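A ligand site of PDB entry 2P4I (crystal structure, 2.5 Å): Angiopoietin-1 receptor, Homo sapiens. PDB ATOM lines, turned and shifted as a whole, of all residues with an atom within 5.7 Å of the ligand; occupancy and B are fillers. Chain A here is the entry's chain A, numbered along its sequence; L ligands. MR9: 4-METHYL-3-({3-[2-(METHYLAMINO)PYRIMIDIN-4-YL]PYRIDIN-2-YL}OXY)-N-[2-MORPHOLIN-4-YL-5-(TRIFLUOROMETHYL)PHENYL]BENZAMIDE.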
ATOM      1  N   VAL A  31       3.747  24.256 -20.943  1.00  0.00           N
ATOM      2  CA  VAL A  31       4.059  23.530 -22.218  1.00  0.00           C
ATOM      3  C   VAL A  31       3.915  24.448 -23.431  1.00  0.00           C
ATOM      4  O   VAL A  31       2.858  25.062 -23.630  1.00  0.00           O
ATOM      5  CB  VAL A  31       3.164  22.279 -22.398  1.00  0.00           C
ATOM      6  CG1 VAL A  31       3.603  21.474 -23.629  1.00  0.00           C
ATOM      7  CG2 VAL A  31       3.199  21.401 -21.144  1.00  0.00           C
ATOM      8  N   ALA A  46       7.184  19.912 -28.534  1.00  0.00           N
ATOM      9  CA  ALA A  46       6.413  20.429 -27.410  1.00  0.00           C
ATOM     10  C   ALA A  46       7.332  20.458 -26.203  1.00  0.00           C
ATOM     11  O   ALA A  46       7.755  19.418 -25.705  1.00  0.00           O
ATOM     12  CB  ALA A  46       5.210  19.555 -27.143  1.00  0.00           C
ATOM     13  N   ILE A  47       7.662  21.677 -25.745  1.00  0.00           N
ATOM     14  CA  ILE A  47       8.674  21.849 -24.700  1.00  0.00           C
ATOM     15  C   ILE A  47       8.053  22.163 -23.341  1.00  0.00           C
ATOM     16  O   ILE A  47       7.195  23.037 -23.226  1.00  0.00           O
ATOM     17  CB  ILE A  47       9.732  22.919 -25.076  1.00  0.00           C
ATOM     18  CG1 ILE A  47      10.401  22.560 -26.404  1.00  0.00           C
ATOM     19  CG2 ILE A  47      10.776  23.042 -23.958  1.00  0.00           C
ATOM     20  CD1 ILE A  47      11.529  23.501 -26.842  1.00  0.00           C
ATOM     21  N   LYS A  48       8.501  21.417 -22.334  1.00  0.00           N
ATOM     22  CA  LYS A  48       8.106  21.623 -20.946  1.00  0.00           C
ATOM     23  C   LYS A  48       9.276  22.229 -20.190  1.00  0.00           C
ATOM     24  O   LYS A  48      10.423  21.835 -20.407  1.00  0.00           O
ATOM     25  CB  LYS A  48       7.724  20.278 -20.329  1.00  0.00           C
ATOM     26  CG  LYS A  48       6.977  20.372 -19.011  1.00  0.00           C
ATOM     27  CD  LYS A  48       6.939  19.013 -18.325  1.00  0.00           C
ATOM     28  CE  LYS A  48       6.179  19.065 -17.015  1.00  0.00           C
ATOM     29  NZ  LYS A  48       6.152  17.725 -16.370  1.00  0.00           N
ATOM     30  N   GLU A  65      12.813  14.472 -14.099  1.00  0.00           N
ATOM     31  CA  GLU A  65      12.004  13.739 -15.069  1.00  0.00           C
ATOM     32  C   GLU A  65      12.839  13.109 -16.195  1.00  0.00           C
ATOM     33  O   GLU A  65      12.378  12.182 -16.875  1.00  0.00           O
ATOM     34  CB  GLU A  65      10.948  14.661 -15.681  1.00  0.00           C
ATOM     35  CG  GLU A  65       9.816  15.060 -14.734  1.00  0.00           C
ATOM     36  CD  GLU A  65       8.755  15.912 -15.408  1.00  0.00           C
ATOM     37  OE1 GLU A  65       7.876  16.448 -14.696  1.00  0.00           O
ATOM     38  OE2 GLU A  65       8.787  16.057 -16.656  1.00  0.00           O
ATOM     39  N   VAL A  68      13.418   9.205 -16.144  1.00  0.00           N
ATOM     40  CA  VAL A  68      12.269   8.383 -16.535  1.00  0.00           C
ATOM     41  C   VAL A  68      12.084   8.348 -18.049  1.00  0.00           C
ATOM     42  O   VAL A  68      11.847   7.286 -18.617  1.00  0.00           O
ATOM     43  CB  VAL A  68      10.967   8.854 -15.827  1.00  0.00           C
ATOM     44  CG1 VAL A  68       9.823   7.885 -16.072  1.00  0.00           C
ATOM     45  CG2 VAL A  68      11.190   8.992 -14.336  1.00  0.00           C
ATOM     46  N   LEU A  69      12.217   9.505 -18.691  1.00  0.00           N
ATOM     47  CA  LEU A  69      12.051   9.595 -20.127  1.00  0.00           C
ATOM     48  C   LEU A  69      13.138   8.814 -20.882  1.00  0.00           C
ATOM     49  O   LEU A  69      12.851   8.117 -21.863  1.00  0.00           O
ATOM     50  CB  LEU A  69      12.025  11.052 -20.566  1.00  0.00           C
ATOM     51  CG  LEU A  69      10.790  11.893 -20.249  1.00  0.00           C
ATOM     52  CD1 LEU A  69      11.071  13.368 -20.520  1.00  0.00           C
ATOM     53  CD2 LEU A  69       9.560  11.447 -21.037  1.00  0.00           C
ATOM     54  N   LEU A  72      12.713   4.972 -20.893  1.00  0.00           N
ATOM     55  CA  LEU A  72      11.639   4.455 -21.734  1.00  0.00           C
ATOM     56  C   LEU A  72      12.165   4.006 -23.103  1.00  0.00           C
ATOM     57  O   LEU A  72      11.537   3.193 -23.779  1.00  0.00           O
ATOM     58  CB  LEU A  72      10.545   5.508 -21.938  1.00  0.00           C
ATOM     59  CG  LEU A  72       9.742   6.033 -20.759  1.00  0.00           C
ATOM     60  CD1 LEU A  72       8.892   7.210 -21.230  1.00  0.00           C
ATOM     61  CD2 LEU A  72       8.870   4.978 -20.086  1.00  0.00           C
ATOM     62  N   ILE A  78       5.117   5.234 -28.628  1.00  0.00           N
ATOM     63  CA  ILE A  78       5.204   6.098 -27.456  1.00  0.00           C
ATOM     64  C   ILE A  78       5.676   7.492 -27.881  1.00  0.00           C
ATOM     65  O   ILE A  78       6.103   7.694 -29.026  1.00  0.00           O
ATOM     66  CB  ILE A  78       6.071   5.473 -26.320  1.00  0.00           C
ATOM     67  CG1 ILE A  78       7.556   5.405 -26.708  1.00  0.00           C
ATOM     68  CG2 ILE A  78       5.540   4.104 -25.944  1.00  0.00           C
ATOM     69  CD1 ILE A  78       8.504   5.009 -25.554  1.00  0.00           C
ATOM     70  N   ILE A  79       5.591   8.449 -26.968  1.00  0.00           N
ATOM     71  CA  ILE A  79       6.174   9.770 -27.203  1.00  0.00           C
ATOM     72  C   ILE A  79       7.701   9.686 -27.352  1.00  0.00           C
ATOM     73  O   ILE A  79       8.336   8.791 -26.800  1.00  0.00           O
ATOM     74  CB  ILE A  79       5.767  10.803 -26.095  1.00  0.00           C
ATOM     75  CG1 ILE A  79       6.053  10.259 -24.696  1.00  0.00           C
ATOM     76  CG2 ILE A  79       4.304  11.223 -26.239  1.00  0.00           C
ATOM     77  CD1 ILE A  79       7.229  10.913 -24.032  1.00  0.00           C
ATOM     78  N   LEU A  93      12.371  20.165 -21.172  1.00  0.00           N
ATOM     79  CA  LEU A  93      12.300  18.855 -21.858  1.00  0.00           C
ATOM     80  C   LEU A  93      11.613  18.948 -23.217  1.00  0.00           C
ATOM     81  O   LEU A  93      10.473  19.416 -23.332  1.00  0.00           O
ATOM     82  CB  LEU A  93      11.615  17.805 -20.977  1.00  0.00           C
ATOM     83  CG  LEU A  93      12.378  17.366 -19.726  1.00  0.00           C
ATOM     84  CD1 LEU A  93      11.440  16.662 -18.741  1.00  0.00           C
ATOM     85  CD2 LEU A  93      13.560  16.463 -20.083  1.00  0.00           C
ATOM     86  N   ILE A  95       9.949  17.192 -26.416  1.00  0.00           N
ATOM     87  CA  ILE A  95       9.335  16.014 -27.038  1.00  0.00           C
ATOM     88  C   ILE A  95       8.701  16.272 -28.420  1.00  0.00           C
ATOM     89  O   ILE A  95       8.083  17.318 -28.634  1.00  0.00           O
ATOM     90  CB  ILE A  95       8.348  15.250 -26.080  1.00  0.00           C
ATOM     91  CG1 ILE A  95       6.933  15.826 -26.149  1.00  0.00           C
ATOM     92  CG2 ILE A  95       8.891  15.157 -24.638  1.00  0.00           C
ATOM     93  CD1 ILE A  95       5.878  14.735 -26.166  1.00  0.00           C
ATOM     94  N   GLU A  96       8.859  15.306 -29.333  1.00  0.00           N
ATOM     95  CA  GLU A  96       8.374  15.436 -30.721  1.00  0.00           C
ATOM     96  C   GLU A  96       6.895  15.785 -30.753  1.00  0.00           C
ATOM     97  O   GLU A  96       6.070  15.061 -30.174  1.00  0.00           O
ATOM     98  CB  GLU A  96       8.656  14.163 -31.550  1.00  0.00           C
ATOM     99  CG  GLU A  96       8.432  14.356 -33.060  1.00  0.00           C
ATOM    100  CD  GLU A  96       8.421  13.041 -33.861  1.00  0.00           C
ATOM    101  OE1 GLU A  96       8.014  13.085 -35.055  1.00  0.00           O
ATOM    102  OE2 GLU A  96       8.807  11.988 -33.314  1.00  0.00           O
ATOM    103  N   TYR A  97       6.576  16.887 -31.428  1.00  0.00           N
ATOM    104  CA  TYR A  97       5.215  17.396 -31.489  1.00  0.00           C
ATOM    105  C   TYR A  97       4.308  16.501 -32.326  1.00  0.00           C
ATOM    106  O   TYR A  97       4.722  15.981 -33.373  1.00  0.00           O
ATOM    107  CB  TYR A  97       5.211  18.814 -32.031  1.00  0.00           C
ATOM    108  CG  TYR A  97       3.883  19.519 -31.984  1.00  0.00           C
ATOM    109  CD1 TYR A  97       3.383  20.022 -30.774  1.00  0.00           C
ATOM    110  CD2 TYR A  97       3.118  19.694 -33.143  1.00  0.00           C
ATOM    111  CE1 TYR A  97       2.148  20.682 -30.725  1.00  0.00           C
ATOM    112  CE2 TYR A  97       1.891  20.359 -33.104  1.00  0.00           C
ATOM    113  CZ  TYR A  97       1.410  20.850 -31.893  1.00  0.00           C
ATOM    114  OH  TYR A  97       0.196  21.512 -31.835  1.00  0.00           O
ATOM    115  N   ALA A  98       3.088  16.309 -31.841  1.00  0.00           N
ATOM    116  CA  ALA A  98       2.074  15.503 -32.528  1.00  0.00           C
ATOM    117  C   ALA A  98       1.060  16.435 -33.198  1.00  0.00           C
ATOM    118  O   ALA A  98       0.254  17.056 -32.497  1.00  0.00           O
ATOM    119  CB  ALA A  98       1.376  14.570 -31.543  1.00  0.00           C
ATOM    120  N   PRO A  99       1.094  16.533 -34.541  1.00  0.00           N
ATOM    121  CA  PRO A  99       0.312  17.581 -35.230  1.00  0.00           C
ATOM    122  C   PRO A  99      -1.186  17.426 -35.060  1.00  0.00           C
ATOM    123  O   PRO A  99      -1.909  18.413 -35.134  1.00  0.00           O
ATOM    124  CB  PRO A  99       0.718  17.431 -36.712  1.00  0.00           C
ATOM    125  CG  PRO A  99       1.948  16.567 -36.723  1.00  0.00           C
ATOM    126  CD  PRO A  99       1.817  15.685 -35.512  1.00  0.00           C
ATOM    127  N   GLY A 101      -2.746  16.327 -32.273  1.00  0.00           N
ATOM    128  CA  GLY A 101      -3.138  16.426 -30.867  1.00  0.00           C
ATOM    129  C   GLY A 101      -3.673  15.136 -30.270  1.00  0.00           C
ATOM    130  O   GLY A 101      -3.468  14.066 -30.837  1.00  0.00           O
ATOM    131  N   ASN A 102      -4.383  15.248 -29.135  1.00  0.00           N
ATOM    132  CA  ASN A 102      -4.879  14.068 -28.421  1.00  0.00           C
ATOM    133  C   ASN A 102      -6.008  13.330 -29.118  1.00  0.00           C
ATOM    134  O   ASN A 102      -6.840  13.935 -29.790  1.00  0.00           O
ATOM    135  CB  ASN A 102      -5.254  14.407 -26.971  1.00  0.00           C
ATOM    136  CG  ASN A 102      -6.559  15.159 -26.865  1.00  0.00           C
ATOM    137  OD1 ASN A 102      -7.631  14.572 -26.970  1.00  0.00           O
ATOM    138  ND2 ASN A 102      -6.470  16.472 -26.638  1.00  0.00           N
ATOM    139  N   LEU A 148       5.748  -0.976 -23.437  1.00  0.00           N
ATOM    140  CA  LEU A 148       5.838  -0.365 -22.115  1.00  0.00           C
ATOM    141  C   LEU A 148       5.667  -1.335 -20.925  1.00  0.00           C
ATOM    142  O   LEU A 148       6.287  -1.148 -19.875  1.00  0.00           O
ATOM    143  CB  LEU A 148       4.878   0.824 -21.995  1.00  0.00           C
ATOM    144  CG  LEU A 148       5.276   2.135 -22.660  1.00  0.00           C
ATOM    145  CD1 LEU A 148       4.248   3.193 -22.410  1.00  0.00           C
ATOM    146  CD2 LEU A 148       6.628   2.597 -22.150  1.00  0.00           C
ATOM    147  N   PHE A 153       6.577  -1.000 -16.824  1.00  0.00           N
ATOM    148  CA  PHE A 153       6.003   0.314 -16.639  1.00  0.00           C
ATOM    149  C   PHE A 153       4.498   0.179 -16.504  1.00  0.00           C
ATOM    150  O   PHE A 153       3.824  -0.507 -17.274  1.00  0.00           O
ATOM    151  CB  PHE A 153       6.375   1.212 -17.815  1.00  0.00           C
ATOM    152  CG  PHE A 153       5.747   2.566 -17.755  1.00  0.00           C
ATOM    153  CD1 PHE A 153       6.391   3.617 -17.093  1.00  0.00           C
ATOM    154  CD2 PHE A 153       4.527   2.816 -18.356  1.00  0.00           C
ATOM    155  CE1 PHE A 153       5.834   4.868 -17.037  1.00  0.00           C
ATOM    156  CE2 PHE A 153       3.961   4.071 -18.305  1.00  0.00           C
ATOM    157  CZ  PHE A 153       4.619   5.101 -17.639  1.00  0.00           C
ATOM    158  N   HIS A 155       1.113   2.382 -16.356  1.00  0.00           N
ATOM    159  CA  HIS A 155       0.616   3.687 -16.729  1.00  0.00           C
ATOM    160  C   HIS A 155      -0.333   4.236 -15.683  1.00  0.00           C
ATOM    161  O   HIS A 155      -0.107   5.337 -15.187  1.00  0.00           O
ATOM    162  CB  HIS A 155      -0.059   3.674 -18.103  1.00  0.00           C
ATOM    163  CG  HIS A 155      -0.151   5.017 -18.740  1.00  0.00           C
ATOM    164  ND1 HIS A 155      -1.031   5.992 -18.303  1.00  0.00           N
ATOM    165  CD2 HIS A 155       0.529   5.568 -19.771  1.00  0.00           C
ATOM    166  CE1 HIS A 155      -0.893   7.073 -19.048  1.00  0.00           C
ATOM    167  NE2 HIS A 155       0.046   6.838 -19.954  1.00  0.00           N
ATOM    168  N   LEU A 164      -1.596  10.389 -28.044  1.00  0.00           N
ATOM    169  CA  LEU A 164      -1.346  11.395 -29.074  1.00  0.00           C
ATOM    170  C   LEU A 164      -1.457  10.814 -30.480  1.00  0.00           C
ATOM    171  O   LEU A 164      -1.176   9.632 -30.711  1.00  0.00           O
ATOM    172  CB  LEU A 164       0.007  12.079 -28.839  1.00  0.00           C
ATOM    173  CG  LEU A 164       0.093  13.107 -27.687  1.00  0.00           C
ATOM    174  CD1 LEU A 164       1.520  13.453 -27.375  1.00  0.00           C
ATOM    175  CD2 LEU A 164      -0.698  14.389 -27.959  1.00  0.00           C
ATOM    176  N   ILE A 173       1.396   6.639 -26.933  1.00  0.00           N
ATOM    177  CA  ILE A 173       1.105   6.752 -25.515  1.00  0.00           C
ATOM    178  C   ILE A 173       1.788   7.994 -24.955  1.00  0.00           C
ATOM    179  O   ILE A 173       2.958   8.266 -25.226  1.00  0.00           O
ATOM    180  CB  ILE A 173       1.601   5.514 -24.699  1.00  0.00           C
ATOM    181  CG1 ILE A 173       1.433   4.192 -25.480  1.00  0.00           C
ATOM    182  CG2 ILE A 173       0.955   5.483 -23.289  1.00  0.00           C
ATOM    183  CD1 ILE A 173       0.021   3.719 -25.629  1.00  0.00           C
ATOM    184  N   ALA A 174       1.048   8.750 -24.161  1.00  0.00           N
ATOM    185  CA  ALA A 174       1.612   9.843 -23.423  1.00  0.00           C
ATOM    186  C   ALA A 174       1.051   9.809 -22.011  1.00  0.00           C
ATOM    187  O   ALA A 174       0.173   8.999 -21.687  1.00  0.00           O
ATOM    188  CB  ALA A 174       1.304  11.167 -24.095  1.00  0.00           C
ATOM    189  N   ASP A 175       1.590  10.691 -21.168  1.00  0.00           N
ATOM    190  CA  ASP A 175       1.145  10.861 -19.808  1.00  0.00           C
ATOM    191  C   ASP A 175       1.301  12.350 -19.520  1.00  0.00           C
ATOM    192  O   ASP A 175       2.417  12.868 -19.493  1.00  0.00           O
ATOM    193  CB  ASP A 175       1.963  10.025 -18.827  1.00  0.00           C
ATOM    194  CG  ASP A 175       1.630  10.329 -17.366  1.00  0.00           C
ATOM    195  OD1 ASP A 175       0.793  11.197 -17.073  1.00  0.00           O
ATOM    196  OD2 ASP A 175       2.220   9.681 -16.490  1.00  0.00           O
ATOM    197  N   PHE A 176       0.169  13.006 -19.318  1.00  0.00           N
ATOM    198  CA  PHE A 176       0.129  14.439 -19.121  1.00  0.00           C
ATOM    199  C   PHE A 176      -0.068  14.783 -17.645  1.00  0.00           C
ATOM    200  O   PHE A 176      -0.456  15.889 -17.303  1.00  0.00           O
ATOM    201  CB  PHE A 176      -0.963  15.093 -20.008  1.00  0.00           C
ATOM    202  CG  PHE A 176      -0.784  14.835 -21.474  1.00  0.00           C
ATOM    203  CD1 PHE A 176      -1.750  14.149 -22.188  1.00  0.00           C
ATOM    204  CD2 PHE A 176       0.348  15.288 -22.147  1.00  0.00           C
ATOM    205  CE1 PHE A 176      -1.613  13.916 -23.552  1.00  0.00           C
ATOM    206  CE2 PHE A 176       0.510  15.060 -23.527  1.00  0.00           C
ATOM    207  CZ  PHE A 176      -0.481  14.369 -24.226  1.00  0.00           C
ATOM    208  N   GLY A 177       0.210  13.810 -16.777  1.00  0.00           N
ATOM    209  CA  GLY A 177       0.403  14.047 -15.347  1.00  0.00           C
ATOM    210  C   GLY A 177       1.756  14.737 -15.246  1.00  0.00           C
ATOM    211  O   GLY A 177       2.396  14.931 -16.274  1.00  0.00           O
ATOM    212  N   LEU A 178       2.213  15.104 -14.054  1.00  0.00           N
ATOM    213  CA  LEU A 178       3.401  15.964 -14.011  1.00  0.00           C
ATOM    214  C   LEU A 178       4.622  15.533 -13.166  1.00  0.00           C
ATOM    215  O   LEU A 178       5.486  16.356 -12.848  1.00  0.00           O
ATOM    216  CB  LEU A 178       3.017  17.442 -13.707  1.00  0.00           C
ATOM    217  N   SER A 179       4.709  14.240 -12.841  1.00  0.00           N
ATOM    218  CA  SER A 179       5.933  13.684 -12.267  1.00  0.00           C
ATOM    219  C   SER A 179       5.927  12.159 -12.260  1.00  0.00           C
ATOM    220  O   SER A 179       4.883  11.548 -12.031  1.00  0.00           O
ATOM    221  CB  SER A 179       6.156  14.200 -10.842  1.00  0.00           C
ATOM    222  N   ARG A 180       7.091  11.572 -12.541  1.00  0.00           N
ATOM    223  CA  ARG A 180       7.360  10.162 -12.344  1.00  0.00           C
ATOM    224  C   ARG A 180       8.846  10.013 -12.002  1.00  0.00           C
ATOM    225  O   ARG A 180       9.226   9.200 -11.157  1.00  0.00           O
ATOM    226  CB  ARG A 180       7.033   9.354 -13.598  1.00  0.00           C
ATOM    227  CG  ARG A 180       5.580   8.953 -13.752  1.00  0.00           C
ATOM    228  CD  ARG A 180       5.404   7.999 -14.930  1.00  0.00           C
ATOM    229  NE  ARG A 180       4.015   7.938 -15.355  1.00  0.00           N
ATOM    230  CZ  ARG A 180       3.179   6.911 -15.133  1.00  0.00           C
ATOM    231  NH1 ARG A 180       3.604   5.833 -14.485  1.00  0.00           N
ATOM    232  NH2 ARG A 180       1.922   6.983 -15.567  1.00  0.00           N
HETATM  233  C26 MR9 L   1       5.509  11.775 -17.332  1.00  0.00           C
HETATM  234  C27 MR9 L   1       5.835  13.148 -16.737  1.00  0.00           C
HETATM  235  O3  MR9 L   1       7.133  13.124 -16.095  1.00  0.00           O
HETATM  236  C28 MR9 L   1       8.201  12.529 -16.925  1.00  0.00           C
HETATM  237  C29 MR9 L   1       7.826  11.200 -17.610  1.00  0.00           C
HETATM  238  N6  MR9 L   1       6.560  11.453 -18.316  1.00  0.00           N
HETATM  239  C20 MR9 L   1       6.155  10.452 -19.115  1.00  0.00           C
HETATM  240  C21 MR9 L   1       6.233   9.112 -18.711  1.00  0.00           C
HETATM  241  C22 MR9 L   1       5.795   8.108 -19.558  1.00  0.00           C
HETATM  242  C23 MR9 L   1       5.296   8.420 -20.815  1.00  0.00           C
HETATM  243  C25 MR9 L   1       4.785   7.293 -21.716  1.00  0.00           C
HETATM  244  F2  MR9 L   1       3.656   6.873 -21.200  1.00  0.00           F
HETATM  245  F3  MR9 L   1       5.622   6.276 -21.722  1.00  0.00           F
HETATM  246  F1  MR9 L   1       4.533   7.670 -22.972  1.00  0.00           F
HETATM  247  C24 MR9 L   1       5.200   9.747 -21.220  1.00  0.00           C
HETATM  248  C19 MR9 L   1       5.616  10.767 -20.366  1.00  0.00           C
HETATM  249  N4  MR9 L   1       5.598  12.056 -20.779  1.00  0.00           N
HETATM  250  C17 MR9 L   1       4.773  12.632 -21.659  1.00  0.00           C
HETATM  251  O2  MR9 L   1       3.862  12.050 -22.246  1.00  0.00           O
HETATM  252  C12 MR9 L   1       5.071  14.110 -21.973  1.00  0.00           C
HETATM  253  C11 MR9 L   1       4.329  14.736 -22.985  1.00  0.00           C
HETATM  254  C13 MR9 L   1       6.103  14.805 -21.354  1.00  0.00           C
HETATM  255  C14 MR9 L   1       6.362  16.134 -21.694  1.00  0.00           C
HETATM  256  C15 MR9 L   1       5.613  16.768 -22.690  1.00  0.00           C
HETATM  257  C16 MR9 L   1       5.905  18.236 -23.060  1.00  0.00           C
HETATM  258  C10 MR9 L   1       4.584  16.069 -23.316  1.00  0.00           C
HETATM  259  O1  MR9 L   1       3.829  16.649 -24.301  1.00  0.00           O
HETATM  260  C9  MR9 L   1       2.737  17.387 -24.003  1.00  0.00           C
HETATM  261  N3  MR9 L   1       2.482  17.776 -22.741  1.00  0.00           N
HETATM  262  C8  MR9 L   1       1.415  18.507 -22.407  1.00  0.00           C
HETATM  263  C7  MR9 L   1       0.508  18.893 -23.395  1.00  0.00           C
HETATM  264  C6  MR9 L   1       0.756  18.519 -24.714  1.00  0.00           C
HETATM  265  C5  MR9 L   1       1.867  17.741 -25.031  1.00  0.00           C
HETATM  266  C2  MR9 L   1       2.113  17.386 -26.374  1.00  0.00           C
HETATM  267  N1  MR9 L   1       1.270  17.825 -27.325  1.00  0.00           N
HETATM  268  C3  MR9 L   1       3.231  16.636 -26.761  1.00  0.00           C
HETATM  269  C4  MR9 L   1       3.408  16.355 -28.121  1.00  0.00           C
HETATM  270  N2  MR9 L   1       2.536  16.819 -28.989  1.00  0.00           N
HETATM  271  C1  MR9 L   1       1.476  17.543 -28.612  1.00  0.00           C
HETATM  272  N5  MR9 L   1       0.604  17.973 -29.524  1.00  0.00           N
HETATM  273  C18 MR9 L   1      -0.610  18.676 -29.082  1.00  0.00           C
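N of Asp 175 lies within hydrogen-bond range of O2 of the ligand.
N of Ala 98 lies within hydrogen-bond range of N2 of the ligand (2.9 Å).
The backbone carbonyl oxygen (O) of Ala 98 is in hydrogen-bond range of a nitrogen (N5) of the ligand (3.1 Å).
OD2 of Asp 175 lies within salt-bridge range of NE of Arg 180.
O of Leu 148 sits at hydrogen-bond distance from N of Phe 153 (3.1 Å).
O of His 155 lies within hydrogen-bond range of NH2 of Arg 180.
The backbone carbonyl oxygen (O) of Ile 173 is in hydrogen-bond range of the backbone NH (N) of Ile 79.
The side-chain carboxylate of Asp 175 sits at hydrogen-bond distance from the backbone NH of Gly 177, at 2.7 Å.
O of Ile 95 lies within hydrogen-bond range of N of Ala 46 (2.7 Å).
O of Lys 48 is in hydrogen-bond range of N of Leu 93.
The backbone carbonyl oxygen of Ala 174 sits at hydrogen-bond distance from a ring nitrogen (NE2) of His 155 (2.8 Å).
The side-chain carboxylate (OE2) of Glu 65 sits close to an oxygen (O3) of the ligand, 3.4 Å away.
The backbone carbonyl oxygen of Ile 173 sits close to a fluorine (F1) of the ligand, at 2.8 Å.
Val 31 touches the ligand.
O of Ala 46 touches C16 of the ligand (3.4 Å).
Lys 48 touches the ligand (CB to C16, 3.9 Å).
Leu 69 touches the ligand.
CD1 of Leu 72 touches F3 of the ligand, 3.4 Å away.
Ile 79 touches the ligand.
Ile 95 touches the ligand (CD1 to C3, 3.3 Å).
Glu 96 touches the ligand (O to C4, 3.6 Å).
Tyr 97 touches the ligand (CE1 to N5, 3.3 Å).
Gly 101 touches the ligand.
Leu 148 touches the ligand.
CZ of Phe 153 touches C22 of the ligand, 3.8 Å away.
His 155 touches the ligand.
CD1 of Leu 164 touches C4 of the ligand, 3.5 Å away.
Ala 174 touches the ligand.
Phe 176 touches the ligand.
Gly 177 touches the ligand (O to C27, 3.9 Å).
N of Arg 180 touches O3 of the ligand, at 3.9 Å.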
